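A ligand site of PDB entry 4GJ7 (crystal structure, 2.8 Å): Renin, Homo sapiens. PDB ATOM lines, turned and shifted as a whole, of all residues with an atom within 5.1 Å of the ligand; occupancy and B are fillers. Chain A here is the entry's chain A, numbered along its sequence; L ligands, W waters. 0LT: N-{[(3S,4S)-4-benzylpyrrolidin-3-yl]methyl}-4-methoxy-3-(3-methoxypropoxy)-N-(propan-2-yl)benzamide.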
ATOM      1  N   THR A  18      27.124  -3.580  30.881  1.00  0.00           N
ATOM      2  CA  THR A  18      27.048  -3.274  29.466  1.00  0.00           C
ATOM      3  C   THR A  18      27.160  -1.807  29.179  1.00  0.00           C
ATOM      4  O   THR A  18      27.730  -1.448  28.152  1.00  0.00           O
ATOM      5  CB  THR A  18      25.795  -3.891  28.834  1.00  0.00           C
ATOM      6  OG1 THR A  18      24.653  -3.583  29.613  1.00  0.00           O
ATOM      7  CG2 THR A  18      25.891  -5.359  28.682  1.00  0.00           C
ATOM      8  N   GLN A  19      26.609  -0.934  30.039  1.00  0.00           N
ATOM      9  CA  GLN A  19      26.689   0.502  29.765  1.00  0.00           C
ATOM     10  C   GLN A  19      27.242   1.237  30.937  1.00  0.00           C
ATOM     11  O   GLN A  19      26.770   1.034  32.049  1.00  0.00           O
ATOM     12  CB  GLN A  19      25.332   1.103  29.380  1.00  0.00           C
ATOM     13  CG  GLN A  19      24.709   0.476  28.128  1.00  0.00           C
ATOM     14  CD  GLN A  19      23.301   0.899  27.999  1.00  0.00           C
ATOM     15  OE1 GLN A  19      22.969   2.060  28.241  1.00  0.00           O
ATOM     16  NE2 GLN A  19      22.441  -0.034  27.634  1.00  0.00           N
ATOM     17  N   TYR A  20      28.286   2.063  30.674  1.00  0.00           N
ATOM     18  CA  TYR A  20      28.959   2.891  31.668  1.00  0.00           C
ATOM     19  C   TYR A  20      28.872   4.327  31.195  1.00  0.00           C
ATOM     20  O   TYR A  20      29.354   4.666  30.121  1.00  0.00           O
ATOM     21  CB  TYR A  20      30.428   2.470  31.827  1.00  0.00           C
ATOM     22  CG  TYR A  20      30.661   1.098  32.416  1.00  0.00           C
ATOM     23  CD1 TYR A  20      30.568  -0.040  31.630  1.00  0.00           C
ATOM     24  CD2 TYR A  20      31.082   0.946  33.742  1.00  0.00           C
ATOM     25  CE1 TYR A  20      30.807  -1.308  32.153  1.00  0.00           C
ATOM     26  CE2 TYR A  20      31.334  -0.317  34.268  1.00  0.00           C
ATOM     27  CZ  TYR A  20      31.206  -1.438  33.471  1.00  0.00           C
ATOM     28  OH  TYR A  20      31.449  -2.684  33.982  1.00  0.00           O
ATOM     29  N   VAL A  36      28.134   8.686  27.430  1.00  0.00           N
ATOM     30  CA  VAL A  36      29.175   7.672  27.329  1.00  0.00           C
ATOM     31  C   VAL A  36      30.461   8.402  26.968  1.00  0.00           C
ATOM     32  O   VAL A  36      30.462   9.194  26.023  1.00  0.00           O
ATOM     33  CB  VAL A  36      28.829   6.579  26.283  1.00  0.00           C
ATOM     34  CG1 VAL A  36      30.051   5.722  25.958  1.00  0.00           C
ATOM     35  CG2 VAL A  36      27.695   5.720  26.762  1.00  0.00           C
ATOM     36  N   ASP A  38      33.372   7.953  25.166  1.00  0.00           N
ATOM     37  CA  ASP A  38      33.756   7.086  24.044  1.00  0.00           C
ATOM     38  C   ASP A  38      35.123   7.393  23.395  1.00  0.00           C
ATOM     39  O   ASP A  38      35.265   8.423  22.743  1.00  0.00           O
ATOM     40  CB  ASP A  38      32.616   7.145  23.001  1.00  0.00           C
ATOM     41  CG  ASP A  38      32.709   6.184  21.865  1.00  0.00           C
ATOM     42  OD1 ASP A  38      33.447   5.205  21.982  1.00  0.00           O
ATOM     43  OD2 ASP A  38      31.990   6.381  20.863  1.00  0.00           O
ATOM     44  N   GLY A  40      36.339   5.528  21.056  1.00  0.00           N
ATOM     45  CA  GLY A  40      36.113   5.055  19.699  1.00  0.00           C
ATOM     46  C   GLY A  40      35.475   6.065  18.751  1.00  0.00           C
ATOM     47  O   GLY A  40      35.289   5.744  17.577  1.00  0.00           O
ATOM     48  N   SER A  41      35.142   7.281  19.252  1.00  0.00           N
ATOM     49  CA  SER A  41      34.534   8.372  18.476  1.00  0.00           C
ATOM     50  C   SER A  41      35.070   9.725  18.980  1.00  0.00           C
ATOM     51  O   SER A  41      35.685   9.783  20.051  1.00  0.00           O
ATOM     52  CB  SER A  41      33.007   8.302  18.505  1.00  0.00           C
ATOM     53  OG  SER A  41      32.430   8.881  19.657  1.00  0.00           O
ATOM     54  N   TRP A  45      27.672  14.702  21.393  1.00  0.00           N
ATOM     55  CA  TRP A  45      26.288  14.833  20.931  1.00  0.00           C
ATOM     56  C   TRP A  45      25.278  14.448  22.000  1.00  0.00           C
ATOM     57  O   TRP A  45      25.556  13.548  22.787  1.00  0.00           O
ATOM     58  CB  TRP A  45      26.046  14.084  19.616  1.00  0.00           C
ATOM     59  CG  TRP A  45      26.003  12.581  19.716  1.00  0.00           C
ATOM     60  CD1 TRP A  45      26.999  11.723  19.362  1.00  0.00           C
ATOM     61  CD2 TRP A  45      24.873  11.767  20.046  1.00  0.00           C
ATOM     62  NE1 TRP A  45      26.561  10.420  19.474  1.00  0.00           N
ATOM     63  CE2 TRP A  45      25.274  10.415  19.932  1.00  0.00           C
ATOM     64  CE3 TRP A  45      23.566  12.051  20.513  1.00  0.00           C
ATOM     65  CZ2 TRP A  45      24.422   9.348  20.237  1.00  0.00           C
ATOM     66  CZ3 TRP A  45      22.714  10.986  20.787  1.00  0.00           C
ATOM     67  CH2 TRP A  45      23.137   9.660  20.646  1.00  0.00           C
ATOM     68  N   ARG A  82      27.739   7.860  12.040  1.00  0.00           N
ATOM     69  CA  ARG A  82      27.544   6.466  11.646  1.00  0.00           C
ATOM     70  C   ARG A  82      28.371   5.520  12.481  1.00  0.00           C
ATOM     71  O   ARG A  82      29.544   5.283  12.201  1.00  0.00           O
ATOM     72  CB  ARG A  82      27.816   6.258  10.126  1.00  0.00           C
ATOM     73  CG  ARG A  82      26.665   6.614   9.179  1.00  0.00           C
ATOM     74  CD  ARG A  82      27.060   6.654   7.706  1.00  0.00           C
ATOM     75  NE  ARG A  82      26.288   7.657   6.936  1.00  0.00           N
ATOM     76  CZ  ARG A  82      26.676   8.906   6.717  1.00  0.00           C
ATOM     77  NH1 ARG A  82      27.834   9.350   7.192  1.00  0.00           N
ATOM     78  NH2 ARG A  82      25.905   9.733   6.020  1.00  0.00           N
ATOM     79  N   TYR A  83      27.749   4.974  13.513  1.00  0.00           N
ATOM     80  CA  TYR A  83      28.363   3.943  14.328  1.00  0.00           C
ATOM     81  C   TYR A  83      27.935   2.642  13.657  1.00  0.00           C
ATOM     82  O   TYR A  83      27.087   2.661  12.729  1.00  0.00           O
ATOM     83  CB  TYR A  83      27.868   4.018  15.785  1.00  0.00           C
ATOM     84  CG  TYR A  83      28.066   5.377  16.424  1.00  0.00           C
ATOM     85  CD1 TYR A  83      29.339   5.809  16.789  1.00  0.00           C
ATOM     86  CD2 TYR A  83      26.993   6.228  16.649  1.00  0.00           C
ATOM     87  CE1 TYR A  83      29.523   7.042  17.419  1.00  0.00           C
ATOM     88  CE2 TYR A  83      27.171   7.464  17.267  1.00  0.00           C
ATOM     89  CZ  TYR A  83      28.439   7.863  17.664  1.00  0.00           C
ATOM     90  OH  TYR A  83      28.634   9.071  18.257  1.00  0.00           O
ATOM     91  N   SER A  84      28.511   1.536  14.056  1.00  0.00           N
ATOM     92  CA  SER A  84      28.132   0.340  13.331  1.00  0.00           C
ATOM     93  C   SER A  84      27.015  -0.459  14.021  1.00  0.00           C
ATOM     94  O   SER A  84      26.567  -1.499  13.528  1.00  0.00           O
ATOM     95  CB  SER A  84      29.368  -0.460  12.912  1.00  0.00           C
ATOM     96  OG  SER A  84      30.149   0.350  12.052  1.00  0.00           O
ATOM     97  N   THR A  85      26.526   0.095  15.118  1.00  0.00           N
ATOM     98  CA  THR A  85      25.412  -0.426  15.909  1.00  0.00           C
ATOM     99  C   THR A  85      24.121   0.300  15.517  1.00  0.00           C
ATOM    100  O   THR A  85      23.018  -0.211  15.808  1.00  0.00           O
ATOM    101  CB  THR A  85      25.702  -0.231  17.417  1.00  0.00           C
ATOM    102  OG1 THR A  85      26.334   1.048  17.629  1.00  0.00           O
ATOM    103  CG2 THR A  85      26.584  -1.325  18.005  1.00  0.00           C
ATOM    104  N   PRO A 118      19.680   1.310  18.204  1.00  0.00           N
ATOM    105  CA  PRO A 118      19.744   0.791  19.575  1.00  0.00           C
ATOM    106  C   PRO A 118      19.341   1.767  20.707  1.00  0.00           C
ATOM    107  O   PRO A 118      19.354   1.381  21.876  1.00  0.00           O
ATOM    108  CB  PRO A 118      21.220   0.446  19.721  1.00  0.00           C
ATOM    109  CG  PRO A 118      21.922   1.542  18.937  1.00  0.00           C
ATOM    110  CD  PRO A 118      20.954   1.979  17.853  1.00  0.00           C
ATOM    111  N   PHE A 119      19.022   3.010  20.381  1.00  0.00           N
ATOM    112  CA  PHE A 119      18.794   4.050  21.376  1.00  0.00           C
ATOM    113  C   PHE A 119      17.651   3.890  22.380  1.00  0.00           C
ATOM    114  O   PHE A 119      17.693   4.540  23.407  1.00  0.00           O
ATOM    115  CB  PHE A 119      18.932   5.468  20.764  1.00  0.00           C
ATOM    116  CG  PHE A 119      20.273   5.592  20.055  1.00  0.00           C
ATOM    117  CD1 PHE A 119      21.445   5.705  20.784  1.00  0.00           C
ATOM    118  CD2 PHE A 119      20.362   5.470  18.683  1.00  0.00           C
ATOM    119  CE1 PHE A 119      22.691   5.722  20.155  1.00  0.00           C
ATOM    120  CE2 PHE A 119      21.615   5.496  18.046  1.00  0.00           C
ATOM    121  CZ  PHE A 119      22.764   5.618  18.788  1.00  0.00           C
ATOM    122  N   LEU A 121      17.316   1.230  24.037  1.00  0.00           N
ATOM    123  CA  LEU A 121      18.050   0.365  24.955  1.00  0.00           C
ATOM    124  C   LEU A 121      19.140   1.119  25.685  1.00  0.00           C
ATOM    125  O   LEU A 121      19.738   0.583  26.637  1.00  0.00           O
ATOM    126  CB  LEU A 121      18.667  -0.791  24.162  1.00  0.00           C
ATOM    127  CG  LEU A 121      17.692  -1.620  23.293  1.00  0.00           C
ATOM    128  CD1 LEU A 121      18.427  -2.542  22.367  1.00  0.00           C
ATOM    129  CD2 LEU A 121      16.686  -2.388  24.153  1.00  0.00           C
ATOM    130  N   ALA A 122      19.424   2.361  25.244  1.00  0.00           N
ATOM    131  CA  ALA A 122      20.448   3.189  25.867  1.00  0.00           C
ATOM    132  C   ALA A 122      19.944   3.773  27.188  1.00  0.00           C
ATOM    133  O   ALA A 122      18.835   4.324  27.240  1.00  0.00           O
ATOM    134  CB  ALA A 122      20.850   4.333  24.933  1.00  0.00           C
ATOM    135  N   PHE A 124      22.047   5.903  28.570  1.00  0.00           N
ATOM    136  CA  PHE A 124      22.663   7.187  28.357  1.00  0.00           C
ATOM    137  C   PHE A 124      21.843   7.967  27.354  1.00  0.00           C
ATOM    138  O   PHE A 124      21.140   7.359  26.537  1.00  0.00           O
ATOM    139  CB  PHE A 124      24.106   7.008  27.854  1.00  0.00           C
ATOM    140  CG  PHE A 124      24.250   6.097  26.647  1.00  0.00           C
ATOM    141  CD1 PHE A 124      24.263   4.717  26.801  1.00  0.00           C
ATOM    142  CD2 PHE A 124      24.432   6.633  25.374  1.00  0.00           C
ATOM    143  CE1 PHE A 124      24.423   3.878  25.690  1.00  0.00           C
ATOM    144  CE2 PHE A 124      24.600   5.790  24.266  1.00  0.00           C
ATOM    145  CZ  PHE A 124      24.606   4.423  24.427  1.00  0.00           C
ATOM    146  N   VAL A 127      26.705  11.099  23.858  1.00  0.00           N
ATOM    147  CA  VAL A 127      28.099  10.644  23.806  1.00  0.00           C
ATOM    148  C   VAL A 127      29.068  11.805  23.921  1.00  0.00           C
ATOM    149  O   VAL A 127      28.808  12.861  23.382  1.00  0.00           O
ATOM    150  CB  VAL A 127      28.348   9.851  22.469  1.00  0.00           C
ATOM    151  CG1 VAL A 127      29.791   9.379  22.349  1.00  0.00           C
ATOM    152  CG2 VAL A 127      27.379   8.671  22.324  1.00  0.00           C
ATOM    153  N   TYR A 162      36.489   0.868  35.064  1.00  0.00           N
ATOM    154  CA  TYR A 162      35.139   0.340  34.921  1.00  0.00           C
ATOM    155  C   TYR A 162      35.009  -0.797  35.929  1.00  0.00           C
ATOM    156  O   TYR A 162      35.734  -1.783  35.833  1.00  0.00           O
ATOM    157  CB  TYR A 162      34.911  -0.227  33.496  1.00  0.00           C
ATOM    158  CG  TYR A 162      34.580   0.751  32.394  1.00  0.00           C
ATOM    159  CD1 TYR A 162      34.345   2.097  32.666  1.00  0.00           C
ATOM    160  CD2 TYR A 162      34.469   0.319  31.071  1.00  0.00           C
ATOM    161  CE1 TYR A 162      34.014   2.990  31.642  1.00  0.00           C
ATOM    162  CE2 TYR A 162      34.134   1.203  30.046  1.00  0.00           C
ATOM    163  CZ  TYR A 162      33.881   2.532  30.345  1.00  0.00           C
ATOM    164  OH  TYR A 162      33.531   3.399  29.338  1.00  0.00           O
ATOM    165  N   LEU A 224      41.578  -1.888  18.676  1.00  0.00           N
ATOM    166  CA  LEU A 224      41.032  -0.580  19.042  1.00  0.00           C
ATOM    167  C   LEU A 224      40.564  -0.620  20.524  1.00  0.00           C
ATOM    168  O   LEU A 224      39.814  -1.522  20.915  1.00  0.00           O
ATOM    169  CB  LEU A 224      39.867  -0.175  18.109  1.00  0.00           C
ATOM    170  CG  LEU A 224      39.207   1.184  18.405  1.00  0.00           C
ATOM    171  CD1 LEU A 224      40.132   2.352  18.074  1.00  0.00           C
ATOM    172  CD2 LEU A 224      37.942   1.318  17.665  1.00  0.00           C
ATOM    173  N   ASP A 226      38.289   0.762  22.863  1.00  0.00           N
ATOM    174  CA  ASP A 226      37.001   1.443  22.809  1.00  0.00           C
ATOM    175  C   ASP A 226      36.232   1.429  24.143  1.00  0.00           C
ATOM    176  O   ASP A 226      35.541   0.451  24.453  1.00  0.00           O
ATOM    177  CB  ASP A 226      36.144   0.803  21.705  1.00  0.00           C
ATOM    178  CG  ASP A 226      35.049   1.643  21.116  1.00  0.00           C
ATOM    179  OD1 ASP A 226      34.763   2.718  21.681  1.00  0.00           O
ATOM    180  OD2 ASP A 226      34.476   1.238  20.088  1.00  0.00           O
ATOM    181  N   THR A 227      36.278   2.551  24.873  1.00  0.00           N
ATOM    182  CA  THR A 227      35.590   2.703  26.150  1.00  0.00           C
ATOM    183  C   THR A 227      34.058   2.801  25.968  1.00  0.00           C
ATOM    184  O   THR A 227      33.303   2.625  26.948  1.00  0.00           O
ATOM    185  CB  THR A 227      36.122   3.900  26.912  1.00  0.00           C
ATOM    186  OG1 THR A 227      35.933   5.050  26.097  1.00  0.00           O
ATOM    187  CG2 THR A 227      37.588   3.785  27.262  1.00  0.00           C
ATOM    188  N   GLY A 228      33.632   3.070  24.728  1.00  0.00           N
ATOM    189  CA  GLY A 228      32.233   3.210  24.356  1.00  0.00           C
ATOM    190  C   GLY A 228      31.567   1.921  23.955  1.00  0.00           C
ATOM    191  O   GLY A 228      30.367   1.900  23.685  1.00  0.00           O
ATOM    192  N   ALA A 229      32.331   0.831  23.929  1.00  0.00           N
ATOM    193  CA  ALA A 229      31.899  -0.504  23.531  1.00  0.00           C
ATOM    194  C   ALA A 229      31.661  -1.365  24.752  1.00  0.00           C
ATOM    195  O   ALA A 229      32.474  -1.378  25.690  1.00  0.00           O
ATOM    196  CB  ALA A 229      32.959  -1.130  22.649  1.00  0.00           C
ATOM    197  N   SER A 230      30.570  -2.120  24.745  1.00  0.00           N
ATOM    198  CA  SER A 230      30.269  -2.986  25.874  1.00  0.00           C
ATOM    199  C   SER A 230      31.206  -4.191  25.961  1.00  0.00           C
ATOM    200  O   SER A 230      31.560  -4.601  27.059  1.00  0.00           O
ATOM    201  CB  SER A 230      28.824  -3.487  25.805  1.00  0.00           C
ATOM    202  OG  SER A 230      27.894  -2.426  25.686  1.00  0.00           O
ATOM    203  N   MET A 303      31.878  -7.773  15.474  1.00  0.00           N
ATOM    204  CA  MET A 303      31.725  -6.372  15.108  1.00  0.00           C
ATOM    205  C   MET A 303      32.684  -6.044  13.964  1.00  0.00           C
ATOM    206  O   MET A 303      33.924  -6.063  14.091  1.00  0.00           O
ATOM    207  CB  MET A 303      31.945  -5.471  16.335  1.00  0.00           C
ATOM    208  CG  MET A 303      32.144  -4.033  16.025  1.00  0.00           C
ATOM    209  SD  MET A 303      30.601  -3.197  15.747  1.00  0.00           S
ATOM    210  CE  MET A 303      30.154  -2.780  17.473  1.00  0.00           C
ATOM    211  N   ILE A 305      34.020  -3.437  12.015  1.00  0.00           N
ATOM    212  CA  ILE A 305      34.300  -2.005  11.941  1.00  0.00           C
ATOM    213  C   ILE A 305      34.779  -1.784  10.494  1.00  0.00           C
ATOM    214  O   ILE A 305      35.554  -2.596   9.963  1.00  0.00           O
ATOM    215  CB  ILE A 305      35.302  -1.567  13.039  1.00  0.00           C
ATOM    216  CG1 ILE A 305      34.634  -1.637  14.439  1.00  0.00           C
ATOM    217  CG2 ILE A 305      35.869  -0.169  12.794  1.00  0.00           C
ATOM    218  CD1 ILE A 305      35.336  -2.542  15.359  1.00  0.00           C
ATOM    219  N   PRO A 306      34.214  -0.756   9.809  1.00  0.00           N
ATOM    220  CA  PRO A 306      34.572  -0.546   8.388  1.00  0.00           C
ATOM    221  C   PRO A 306      35.907   0.166   8.201  1.00  0.00           C
ATOM    222  O   PRO A 306      36.340   0.848   9.129  1.00  0.00           O
ATOM    223  CB  PRO A 306      33.417   0.325   7.884  1.00  0.00           C
ATOM    224  CG  PRO A 306      33.016   1.138   9.078  1.00  0.00           C
ATOM    225  CD  PRO A 306      33.241   0.247  10.278  1.00  0.00           C
ATOM    226  N   THR A 309      39.714   2.437   9.900  1.00  0.00           N
ATOM    227  CA  THR A 309      39.920   1.917  11.263  1.00  0.00           C
ATOM    228  C   THR A 309      39.819   0.414  11.293  1.00  0.00           C
ATOM    229  O   THR A 309      40.694  -0.241  11.876  1.00  0.00           O
ATOM    230  CB  THR A 309      38.941   2.558  12.275  1.00  0.00           C
ATOM    231  OG1 THR A 309      38.932   3.972  12.089  1.00  0.00           O
ATOM    232  CG2 THR A 309      39.276   2.235  13.730  1.00  0.00           C
ATOM    233  N   ALA A 317      34.384  -2.616  27.385  1.00  0.00           N
ATOM    234  CA  ALA A 317      34.203  -2.713  28.834  1.00  0.00           C
ATOM    235  C   ALA A 317      34.654  -4.078  29.418  1.00  0.00           C
ATOM    236  O   ALA A 317      35.243  -4.077  30.515  1.00  0.00           O
ATOM    237  CB  ALA A 317      32.785  -2.380  29.222  1.00  0.00           C
HETATM  238  C1  0LT L   1      27.701   2.280  20.572  1.00  0.00           C
HETATM  239  N2  0LT L   1      28.379   3.473  20.520  1.00  0.00           N
HETATM  240  C3  0LT L   1      29.424   3.694  19.481  1.00  0.00           C
HETATM  241  C4  0LT L   1      26.614   1.908  21.542  1.00  0.00           C
HETATM  242  C5  0LT L   1      30.542   2.626  19.313  1.00  0.00           C
HETATM  243  C6  0LT L   1      26.997   1.531  22.848  1.00  0.00           C
HETATM  244  C7  0LT L   1      26.020   1.056  23.753  1.00  0.00           C
HETATM  245  N8  0LT L   1      32.612   3.548  20.111  1.00  0.00           N
HETATM  246  C9  0LT L   1      31.459   2.915  18.095  1.00  0.00           C
HETATM  247  O10 0LT L   1      27.988   1.293  19.897  1.00  0.00           O
HETATM  248  C11 0LT L   1      24.665   0.925  23.325  1.00  0.00           C
HETATM  249  C12 0LT L   1      25.286   1.753  21.103  1.00  0.00           C
HETATM  250  C13 0LT L   1      32.092   1.677  17.374  1.00  0.00           C
HETATM  251  C14 0LT L   1      27.924   4.629  21.321  1.00  0.00           C
HETATM  252  C15 0LT L   1      24.308   1.291  21.997  1.00  0.00           C
HETATM  253  C16 0LT L   1      31.554   2.584  20.483  1.00  0.00           C
HETATM  254  C17 0LT L   1      32.399   3.985  18.709  1.00  0.00           C
HETATM  255  O18 0LT L   1      26.346   0.685  25.061  1.00  0.00           O
HETATM  256  C19 0LT L   1      33.081   2.129  16.295  1.00  0.00           C
HETATM  257  O20 0LT L   1      23.724   0.401  24.224  1.00  0.00           O
HETATM  258  C21 0LT L   1      27.991   2.185  26.251  1.00  0.00           C
HETATM  259  O22 0LT L   1      29.508   1.332  27.991  1.00  0.00           O
HETATM  260  C23 0LT L   1      27.674   0.780  25.651  1.00  0.00           C
HETATM  261  C24 0LT L   1      29.398   2.279  26.918  1.00  0.00           C
HETATM  262  C25 0LT L   1      28.749   5.176  22.515  1.00  0.00           C
HETATM  263  C26 0LT L   1      27.033   5.616  20.494  1.00  0.00           C
HETATM  264  C27 0LT L   1      34.442   2.392  16.593  1.00  0.00           C
HETATM  265  C28 0LT L   1      32.623   2.321  14.966  1.00  0.00           C
HETATM  266  C29 0LT L   1      22.307   0.430  23.945  1.00  0.00           C
HETATM  267  C30 0LT L   1      30.750   0.600  28.000  1.00  0.00           C
HETATM  268  C31 0LT L   1      35.319   2.868  15.603  1.00  0.00           C
HETATM  269  C32 0LT L   1      33.503   2.783  13.978  1.00  0.00           C
HETATM  270  C33 0LT L   1      34.850   3.029  14.293  1.00  0.00           C
HETATM  271  O   HOH W   1      29.577  -1.042  20.471  1.00  0.00           O
HETATM  272  O   HOH W   2      37.834   5.000  16.401  1.00  0.00           O
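The side-chain carboxylate of Asp 38 lies within salt-bridge range of a nitrogen (N8) of the ligand, at 2.6 Å. The side-chain carboxylate (OD1) of Asp 226 lies within salt-bridge range of a nitrogen (N8) of the ligand. OG1 of Thr 85 is in hydrogen-bond range of O10 of the ligand (2.8 Å). An oxygen (O22) of the ligand is in hydrogen-bond range of the backbone NH of Tyr 20, 3.0 Å away.
OD1 of Asp 38 is in hydrogen-bond range of N of Gly 40, 3.1 Å away. OG of Ser 41 lies within hydrogen-bond range of OD2 of Asp 38 (2.8 Å). OD1 of Asp 226 lies close to N of Gly 228 (3.3 Å). The side-chain carboxylate (OD1) of Asp 226 is in hydrogen-bond range of the backbone NH (N) of Gly 40. OG of Ser 230 is in hydrogen-bond range of O of Thr 18 (2.7 Å). NE1 of Trp 45 sits at hydrogen-bond distance from OH of Tyr 83. The backbone NH (N) of Ala 317 is in hydrogen-bond range of the backbone carbonyl oxygen (O) of Ala 229 (2.8 Å). N of Val 127 lies within hydrogen-bond range of O of Trp 45 (2.9 Å).
An oxygen (O22) of the ligand sits close to the backbone carbonyl oxygen of Thr 18, at 3.3 Å. Gln 19 touches the ligand (CA to O22, 3.4 Å). Val 36 touches the ligand (CG2 to C21, 3.6 Å). Gly 40 touches the ligand. Tyr 83 touches the ligand. O of Pro 118 touches C29 of the ligand, 3.7 Å away. Leu 121 touches the ligand. N of Ala 122 touches C29 of the ligand, at 3.7 Å. Phe 124 touches the ligand (CZ to C11, 3.7 Å). Val 127 touches the ligand. Leu 224 touches the ligand. O of Thr 227 touches C30 of the ligand, at 3.4 Å. Gly 228 touches the ligand (O to C24, 3.4 Å). Ala 229 touches the ligand (O to C30, 3.5 Å). Ser 230 touches the ligand. Ile 305 touches the ligand (CG2 to C33, 3.7 Å). Ala 317 touches the ligand (CB to C30, 3.8 Å). Hydrophobic or aromatic side chains that line the ligand: Tyr 20, Val 36, Tyr 83, Pro 118, Leu 121, Phe 124, Val 127, Leu 224, Ile 305 and Ala 317. The nearest printed residue that does not touch the ligand is Tyr 162 (4.0001 Å).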
